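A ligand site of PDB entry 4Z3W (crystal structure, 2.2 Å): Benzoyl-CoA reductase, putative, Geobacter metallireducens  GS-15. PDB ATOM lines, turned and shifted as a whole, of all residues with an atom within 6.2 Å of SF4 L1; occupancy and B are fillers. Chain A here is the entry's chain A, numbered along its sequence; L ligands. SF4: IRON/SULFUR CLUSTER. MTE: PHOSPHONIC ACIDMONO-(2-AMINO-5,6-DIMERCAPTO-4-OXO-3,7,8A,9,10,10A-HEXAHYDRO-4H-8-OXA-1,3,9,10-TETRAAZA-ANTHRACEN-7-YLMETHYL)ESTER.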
ATOM      1  N   GLY A  74      34.850  13.120  14.206  1.00  0.00           N
ATOM      2  CA  GLY A  74      33.761  12.309  13.717  1.00  0.00           C
ATOM      3  C   GLY A  74      33.705  12.110  12.214  1.00  0.00           C
ATOM      4  O   GLY A  74      32.769  11.510  11.679  1.00  0.00           O
ATOM      5  N   CYS A  75      34.713  12.610  11.506  1.00  0.00           N
ATOM      6  CA  CYS A  75      34.728  12.442  10.052  1.00  0.00           C
ATOM      7  C   CYS A  75      35.369  11.119   9.649  1.00  0.00           C
ATOM      8  O   CYS A  75      36.556  11.071   9.393  1.00  0.00           O
ATOM      9  CB  CYS A  75      35.455  13.611   9.379  1.00  0.00           C
ATOM     10  SG  CYS A  75      35.150  13.682   7.576  1.00  0.00           S
ATOM     11  N   ASN A  76      34.562  10.066   9.558  1.00  0.00           N
ATOM     12  CA  ASN A  76      35.091   8.709   9.434  1.00  0.00           C
ATOM     13  C   ASN A  76      34.245   7.761   8.593  1.00  0.00           C
ATOM     14  O   ASN A  76      34.453   6.534   8.611  1.00  0.00           O
ATOM     15  CB  ASN A  76      35.256   8.122  10.838  1.00  0.00           C
ATOM     16  CG  ASN A  76      34.009   8.323  11.694  1.00  0.00           C
ATOM     17  OD1 ASN A  76      32.895   8.155  11.205  1.00  0.00           O
ATOM     18  ND2 ASN A  76      34.187   8.721  12.942  1.00  0.00           N
ATOM     19  N   ARG A  77      33.303   8.323   7.842  1.00  0.00           N
ATOM     20  CA  ARG A  77      32.303   7.505   7.167  1.00  0.00           C
ATOM     21  C   ARG A  77      32.747   6.913   5.839  1.00  0.00           C
ATOM     22  O   ARG A  77      33.387   7.571   5.004  1.00  0.00           O
ATOM     23  CB  ARG A  77      31.013   8.323   6.948  1.00  0.00           C
ATOM     24  CG  ARG A  77      29.852   7.883   7.855  1.00  0.00           C
ATOM     25  CD  ARG A  77      30.148   8.101   9.351  1.00  0.00           C
ATOM     26  NE  ARG A  77      29.168   7.398  10.179  1.00  0.00           N
ATOM     27  CZ  ARG A  77      29.265   7.190  11.495  1.00  0.00           C
ATOM     28  NH1 ARG A  77      30.319   7.646  12.189  1.00  0.00           N
ATOM     29  NH2 ARG A  77      28.310   6.520  12.122  1.00  0.00           N
ATOM     30  N   GLY A  96      30.152   3.757   9.701  1.00  0.00           N
ATOM     31  CA  GLY A  96      31.042   4.488  10.576  1.00  0.00           C
ATOM     32  C   GLY A  96      32.322   3.727  10.932  1.00  0.00           C
ATOM     33  O   GLY A  96      32.906   3.012  10.117  1.00  0.00           O
ATOM     34  N   GLY A  97      32.778   3.905  12.168  1.00  0.00           N
ATOM     35  CA  GLY A  97      33.935   3.177  12.677  1.00  0.00           C
ATOM     36  C   GLY A  97      35.289   3.720  12.261  1.00  0.00           C
ATOM     37  O   GLY A  97      35.597   4.900  12.453  1.00  0.00           O
ATOM     38  N   ARG A 181      31.968  -1.829  15.173  1.00  0.00           N
ATOM     39  CA  ARG A 181      30.726  -1.212  15.683  1.00  0.00           C
ATOM     40  C   ARG A 181      29.990  -0.417  14.577  1.00  0.00           C
ATOM     41  O   ARG A 181      29.259   0.543  14.846  1.00  0.00           O
ATOM     42  CB  ARG A 181      31.040  -0.313  16.892  1.00  0.00           C
ATOM     43  CG  ARG A 181      31.336   1.170  16.600  1.00  0.00           C
ATOM     44  CD  ARG A 181      30.761   2.026  17.722  1.00  0.00           C
ATOM     45  NE  ARG A 181      30.384   3.382  17.328  1.00  0.00           N
ATOM     46  CZ  ARG A 181      29.232   3.708  16.753  1.00  0.00           C
ATOM     47  NH1 ARG A 181      28.967   4.972  16.418  1.00  0.00           N
ATOM     48  NH2 ARG A 181      28.345   2.774  16.485  1.00  0.00           N
ATOM     49  N   LEU A 246      23.880  15.709  20.851  1.00  0.00           N
ATOM     50  CA  LEU A 246      24.622  15.343  19.660  1.00  0.00           C
ATOM     51  C   LEU A 246      24.723  13.837  19.506  1.00  0.00           C
ATOM     52  O   LEU A 246      24.428  13.087  20.442  1.00  0.00           O
ATOM     53  CB  LEU A 246      26.027  15.966  19.700  1.00  0.00           C
ATOM     54  CG  LEU A 246      26.024  17.496  19.767  1.00  0.00           C
ATOM     55  CD1 LEU A 246      27.414  18.060  19.583  1.00  0.00           C
ATOM     56  CD2 LEU A 246      25.073  18.049  18.686  1.00  0.00           C
ATOM     57  N   GLY A 247      25.122  13.389  18.319  1.00  0.00           N
ATOM     58  CA  GLY A 247      25.356  11.969  18.066  1.00  0.00           C
ATOM     59  C   GLY A 247      24.240  11.277  17.307  1.00  0.00           C
ATOM     60  O   GLY A 247      23.212  11.875  17.017  1.00  0.00           O
ATOM     61  N   SER A 248      24.448  10.011  16.954  1.00  0.00           N
ATOM     62  CA  SER A 248      23.338   9.163  16.530  1.00  0.00           C
ATOM     63  C   SER A 248      22.382   9.058  17.704  1.00  0.00           C
ATOM     64  O   SER A 248      22.797   9.309  18.835  1.00  0.00           O
ATOM     65  CB  SER A 248      23.819   7.779  16.108  1.00  0.00           C
ATOM     66  OG  SER A 248      24.796   7.883  15.084  1.00  0.00           O
ATOM     67  N   GLN A 250      20.872   8.414  20.862  1.00  0.00           N
ATOM     68  CA  GLN A 250      21.642   7.934  21.993  1.00  0.00           C
ATOM     69  C   GLN A 250      20.899   6.840  22.762  1.00  0.00           C
ATOM     70  O   GLN A 250      20.699   6.935  23.951  1.00  0.00           O
ATOM     71  CB  GLN A 250      21.974   9.109  22.915  1.00  0.00           C
ATOM     72  CG  GLN A 250      22.956  10.107  22.315  1.00  0.00           C
ATOM     73  CD  GLN A 250      24.381   9.586  22.323  1.00  0.00           C
ATOM     74  OE1 GLN A 250      24.606   8.435  22.681  1.00  0.00           O
ATOM     75  NE2 GLN A 250      25.339  10.420  21.934  1.00  0.00           N
ATOM     76  N   ILE A 297      31.184   3.028  23.331  1.00  0.00           N
ATOM     77  CA  ILE A 297      32.394   3.229  22.526  1.00  0.00           C
ATOM     78  C   ILE A 297      32.156   4.132  21.317  1.00  0.00           C
ATOM     79  O   ILE A 297      31.052   4.210  20.785  1.00  0.00           O
ATOM     80  CB  ILE A 297      32.954   1.879  22.053  1.00  0.00           C
ATOM     81  CG1 ILE A 297      31.898   1.102  21.262  1.00  0.00           C
ATOM     82  CG2 ILE A 297      33.435   1.053  23.257  1.00  0.00           C
ATOM     83  CD1 ILE A 297      32.432  -0.124  20.606  1.00  0.00           C
ATOM     84  N   SER A 298      33.212   4.828  20.910  1.00  0.00           N
ATOM     85  CA  SER A 298      33.094   5.803  19.821  1.00  0.00           C
ATOM     86  C   SER A 298      33.510   5.250  18.454  1.00  0.00           C
ATOM     87  O   SER A 298      34.087   4.182  18.366  1.00  0.00           O
ATOM     88  CB  SER A 298      33.947   7.028  20.138  1.00  0.00           C
ATOM     89  OG  SER A 298      33.469   7.741  21.270  1.00  0.00           O
ATOM     90  N   CYS A 299      33.180   5.977  17.396  1.00  0.00           N
ATOM     91  CA  CYS A 299      33.815   5.768  16.106  1.00  0.00           C
ATOM     92  C   CYS A 299      35.173   6.481  16.129  1.00  0.00           C
ATOM     93  O   CYS A 299      35.568   7.002  17.163  1.00  0.00           O
ATOM     94  CB  CYS A 299      32.942   6.291  14.965  1.00  0.00           C
ATOM     95  SG  CYS A 299      31.326   5.550  14.947  1.00  0.00           S
ATOM     96  N   TYR A 300      35.847   6.533  14.991  1.00  0.00           N
ATOM     97  CA  TYR A 300      37.163   7.171  14.917  1.00  0.00           C
ATOM     98  C   TYR A 300      37.120   8.647  15.232  1.00  0.00           C
ATOM     99  O   TYR A 300      36.306   9.382  14.667  1.00  0.00           O
ATOM    100  CB  TYR A 300      37.763   6.956  13.539  1.00  0.00           C
ATOM    101  CG  TYR A 300      39.196   7.408  13.397  1.00  0.00           C
ATOM    102  CD1 TYR A 300      40.221   6.783  14.111  1.00  0.00           C
ATOM    103  CD2 TYR A 300      39.543   8.451  12.548  1.00  0.00           C
ATOM    104  CE1 TYR A 300      41.539   7.195  13.982  1.00  0.00           C
ATOM    105  CE2 TYR A 300      40.857   8.871  12.399  1.00  0.00           C
ATOM    106  CZ  TYR A 300      41.855   8.230  13.125  1.00  0.00           C
ATOM    107  OH  TYR A 300      43.159   8.629  12.972  1.00  0.00           O
ATOM    108  N   CYS A 302      36.071  10.558  17.672  1.00  0.00           N
ATOM    109  CA  CYS A 302      34.842  11.176  18.160  1.00  0.00           C
ATOM    110  C   CYS A 302      34.586  10.876  19.634  1.00  0.00           C
ATOM    111  O   CYS A 302      34.759   9.741  20.086  1.00  0.00           O
ATOM    112  CB  CYS A 302      33.654  10.697  17.331  1.00  0.00           C
ATOM    113  SG  CYS A 302      32.112  11.551  17.755  1.00  0.00           S
ATOM    114  N   PRO A 303      34.124  11.885  20.387  1.00  0.00           N
ATOM    115  CA  PRO A 303      33.894  11.669  21.831  1.00  0.00           C
ATOM    116  C   PRO A 303      32.471  11.239  22.205  1.00  0.00           C
ATOM    117  O   PRO A 303      32.233  10.982  23.378  1.00  0.00           O
ATOM    118  CB  PRO A 303      34.200  13.037  22.423  1.00  0.00           C
ATOM    119  CG  PRO A 303      33.753  13.984  21.359  1.00  0.00           C
ATOM    120  CD  PRO A 303      34.113  13.312  20.046  1.00  0.00           C
ATOM    121  N   MET A 304      31.551  11.135  21.250  1.00  0.00           N
ATOM    122  CA  MET A 304      30.138  10.950  21.597  1.00  0.00           C
ATOM    123  C   MET A 304      29.772   9.508  22.022  1.00  0.00           C
ATOM    124  O   MET A 304      28.705   9.297  22.578  1.00  0.00           O
ATOM    125  CB  MET A 304      29.244  11.368  20.425  1.00  0.00           C
ATOM    126  CG  MET A 304      29.361  12.823  20.033  1.00  0.00           C
ATOM    127  SD  MET A 304      29.286  13.947  21.433  1.00  0.00           S
ATOM    128  CE  MET A 304      27.601  13.692  22.035  1.00  0.00           C
ATOM    129  N   LYS A 305      30.659   8.552  21.756  1.00  0.00           N
ATOM    130  CA  LYS A 305      30.464   7.126  22.094  1.00  0.00           C
ATOM    131  C   LYS A 305      28.997   6.663  22.062  1.00  0.00           C
ATOM    132  O   LYS A 305      28.445   6.195  23.055  1.00  0.00           O
ATOM    133  CB  LYS A 305      31.078   6.810  23.482  1.00  0.00           C
ATOM    134  CG  LYS A 305      30.813   7.857  24.566  1.00  0.00           C
ATOM    135  CD  LYS A 305      31.417   7.423  25.887  1.00  0.00           C
ATOM    136  CE  LYS A 305      31.173   8.472  26.979  1.00  0.00           C
ATOM    137  NZ  LYS A 305      31.679   8.047  28.313  1.00  0.00           N
ATOM    138  N   CYS A 306      28.388   6.783  20.882  1.00  0.00           N
ATOM    139  CA  CYS A 306      27.000   6.427  20.624  1.00  0.00           C
ATOM    140  C   CYS A 306      26.711   4.939  20.744  1.00  0.00           C
ATOM    141  O   CYS A 306      25.633   4.535  21.179  1.00  0.00           O
ATOM    142  CB  CYS A 306      26.609   6.881  19.232  1.00  0.00           C
ATOM    143  SG  CYS A 306      26.831   8.631  19.064  1.00  0.00           S
ATOM    144  N   GLY A 307      27.691   4.132  20.345  1.00  0.00           N
ATOM    145  CA  GLY A 307      27.516   2.698  20.289  1.00  0.00           C
ATOM    146  C   GLY A 307      27.917   1.990  21.558  1.00  0.00           C
ATOM    147  O   GLY A 307      28.426   2.594  22.500  1.00  0.00           O
ATOM    148  N   LYS A 321      24.254   0.174  17.949  1.00  0.00           N
ATOM    149  CA  LYS A 321      23.880   1.558  18.201  1.00  0.00           C
ATOM    150  C   LYS A 321      22.468   1.811  17.660  1.00  0.00           C
ATOM    151  O   LYS A 321      21.920   0.986  16.936  1.00  0.00           O
ATOM    152  CB  LYS A 321      24.874   2.521  17.553  1.00  0.00           C
ATOM    153  CG  LYS A 321      24.520   2.974  16.140  1.00  0.00           C
ATOM    154  CD  LYS A 321      24.483   1.815  15.148  1.00  0.00           C
ATOM    155  CE  LYS A 321      25.894   1.210  14.937  1.00  0.00           C
ATOM    156  NZ  LYS A 321      25.903   0.224  13.813  1.00  0.00           N
ATOM    157  N   CYS A 534      30.233  12.276  10.070  1.00  0.00           N
ATOM    158  CA  CYS A 534      29.122  11.577  10.697  1.00  0.00           C
ATOM    159  C   CYS A 534      27.936  12.507  10.911  1.00  0.00           C
ATOM    160  O   CYS A 534      28.070  13.580  11.492  1.00  0.00           O
ATOM    161  CB  CYS A 534      29.526  10.958  12.037  1.00  0.00           C
ATOM    162  SG  CYS A 534      28.154  10.100  12.843  1.00  0.00           S
ATOM    163  N   ALA A 535      26.759  12.089  10.455  1.00  0.00           N
ATOM    164  CA  ALA A 535      25.547  12.909  10.602  1.00  0.00           C
ATOM    165  C   ALA A 535      25.265  13.211  12.077  1.00  0.00           C
ATOM    166  O   ALA A 535      24.491  14.118  12.388  1.00  0.00           O
ATOM    167  CB  ALA A 535      24.385  12.216   9.964  1.00  0.00           C
ATOM    168  N   GLY A 536      25.917  12.464  12.974  1.00  0.00           N
ATOM    169  CA  GLY A 536      25.714  12.604  14.413  1.00  0.00           C
ATOM    170  C   GLY A 536      26.224  13.920  14.951  1.00  0.00           C
ATOM    171  O   GLY A 536      25.836  14.365  16.031  1.00  0.00           O
ATOM    172  N   LEU A 537      27.105  14.559  14.197  1.00  0.00           N
ATOM    173  CA  LEU A 537      27.635  15.842  14.588  1.00  0.00           C
ATOM    174  C   LEU A 537      27.276  16.897  13.556  1.00  0.00           C
ATOM    175  O   LEU A 537      27.810  18.007  13.564  1.00  0.00           O
ATOM    176  CB  LEU A 537      29.156  15.774  14.750  1.00  0.00           C
ATOM    177  CG  LEU A 537      29.728  14.880  15.860  1.00  0.00           C
ATOM    178  CD1 LEU A 537      31.244  14.866  15.779  1.00  0.00           C
ATOM    179  CD2 LEU A 537      29.280  15.366  17.230  1.00  0.00           C
HETATM  180 FE1  SF4 L   1      30.315   7.519  15.859  1.00  0.00          FE
HETATM  181 FE2  SF4 L   1      30.717   9.913  16.982  1.00  0.00          FE
HETATM  182 FE3  SF4 L   1      28.424   8.627  17.428  1.00  0.00          FE
HETATM  183 FE4  SF4 L   1      28.918   9.608  14.937  1.00  0.00          FE
HETATM  184  S1  SF4 L   1      28.595  10.824  16.867  1.00  0.00           S
HETATM  185  S2  SF4 L   1      28.046   7.596  15.383  1.00  0.00           S
HETATM  186  S3  SF4 L   1      31.214   9.352  14.815  1.00  0.00           S
HETATM  187  S4  SF4 L   1      30.507   7.939  18.133  1.00  0.00           S
HETATM  188  N1  MTE L   2      26.450   9.677   8.938  1.00  0.00           N
HETATM  189  C2  MTE L   2      26.263   9.947   7.631  1.00  0.00           C
HETATM  190  N2  MTE L   2      27.270  10.713   6.990  1.00  0.00           N
HETATM  191  N3  MTE L   2      25.141   9.514   6.917  1.00  0.00           N
HETATM  192  C4  MTE L   2      24.198   8.767   7.611  1.00  0.00           C
HETATM  193  O4  MTE L   2      23.184   8.342   7.029  1.00  0.00           O
HETATM  194  N5  MTE L   2      23.469   7.708   9.794  1.00  0.00           N
HETATM  195  C6  MTE L   2      23.500   7.941  11.251  1.00  0.00           C
HETATM  196  C7  MTE L   2      24.899   7.885  11.784  1.00  0.00           C
HETATM  197  N8  MTE L   2      25.815   8.676  11.010  1.00  0.00           N
HETATM  198  C9  MTE L   2      24.428   8.480   9.039  1.00  0.00           C
HETATM  199  C10 MTE L   2      25.513   8.918   9.631  1.00  0.00           C
HETATM  200  C1' MTE L   2      22.651   6.992  12.082  1.00  0.00           C
HETATM  201  S1' MTE L   2      20.925   7.342  12.129  1.00  0.00           S
HETATM  202  C2' MTE L   2      23.252   5.929  12.767  1.00  0.00           C
HETATM  203  S2' MTE L   2      22.274   4.796  13.712  1.00  0.00           S
HETATM  204  C3' MTE L   2      24.745   5.690  12.632  1.00  0.00           C
HETATM  205  O3' MTE L   2      25.319   6.575  11.708  1.00  0.00           O
HETATM  206  C4' MTE L   2      25.015   4.288  12.154  1.00  0.00           C
HETATM  207  O4' MTE L   2      26.397   4.056  12.068  1.00  0.00           O
HETATM  208  P   MTE L   2      26.962   2.879  11.177  1.00  0.00           P
HETATM  209  O1P MTE L   2      26.411   1.499  11.658  1.00  0.00           O
HETATM  210  O2P MTE L   2      28.486   2.900  11.295  1.00  0.00           O
HETATM  211  O3P MTE L   2      26.546   3.156   9.737  1.00  0.00           O
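N of Gly 96 lies within hydrogen-bond range of O2P of MTE L2, at 2.5 Å.
S2 of SF4 L1 lies close to OG of Ser 248, 3.3 Å away.
A nitrogen (N8) of MTE L2 sits close to the side-chain sulfur (SG) of Cys 534, at 3.3 Å.
O2P of MTE L2 is in salt-bridge range of NH2 of Arg 77 (3.7 Å).
FE3 of SF4 L1 is bound by SG of Cys 306.
The side-chain sulfur of Cys 302 binds an iron atom (FE2) of SF4 L1 (2.3 Å).
S4 of SF4 L1 lies close to N of Cys 306, 3.7 Å away.
The backbone NH (N) of Cys 299 lies close to a sulfur (S4) of SF4 L1 (3.4 Å).
SG of Cys 534 binds FE4 of SF4 L1 (2.3 Å).
A nitrogen (N1) of MTE L2 is in hydrogen-bond range of the backbone NH (N) of Ala 535.
The side-chain sulfur (SG) of Cys 299 is bound to an iron atom (FE1) of SF4 L1 (2.4 Å).
The backbone NH (N) of Lys 305 lies close to a sulfur (S4) of SF4 L1, at 3.7 Å.
ND2 of Asn 76 sits close to S3 of SF4 L1.
NH1 of Arg 181 lies close to S2 of SF4 L1 (3.0 Å).
NZ of Lys 321 lies within salt-bridge range of O1P of MTE L2, 2.6 Å away.
The guanidinium group (NH1) of Arg 77 lies close to a sulfur (S3) of SF4 L1, 3.3 Å away.
The guanidinium group (NH1) of Arg 77 lies close to the side-chain sulfur (SG) of Cys 534.
The backbone carbonyl oxygen (O) of Cys 302 is in hydrogen-bond range of the side-chain hydroxyl (OG) of Ser 298 (2.7 Å).
The backbone NH (N) of Cys 534 lies within hydrogen-bond range of the backbone carbonyl oxygen (O) of Gly 74 (3.1 Å).
O of Tyr 300 is in hydrogen-bond range of ND2 of Asn 76 (2.8 Å).
SG of Cys 299 sits close to N of Gly 97 (3.5 Å).
NH1 of Arg 77 sits close to SG of Cys 299 (3.6 Å).
The side-chain amide nitrogen of Asn 76 lies within hydrogen-bond range of the backbone carbonyl oxygen of Gly 74, 3.4 Å away.
The backbone NH of Met 304 sits close to the side-chain sulfur of Cys 302 (3.6 Å).
Gly 247 touches SF4 L1 (CA to S1, 3.6 Å).
Ser 298 touches SF4 L1 (CA to S4, 3.8 Å).
Met 304 touches SF4 L1.
12 residues have an atom within 4 Å of SF4 L1: Asn 76, Arg 77, Arg 181, Gly 247, Ser 248, Ser 298, Cys 299, Cys 302, Met 304, Lys 305, Cys 306 and Cys 534.
Along chain A the residues within 4 Å of SF4 L1 span positions 76 to 534.
The nearest printed residue that does not touch SF4 L1 is Gly 74 (4.1 Å).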
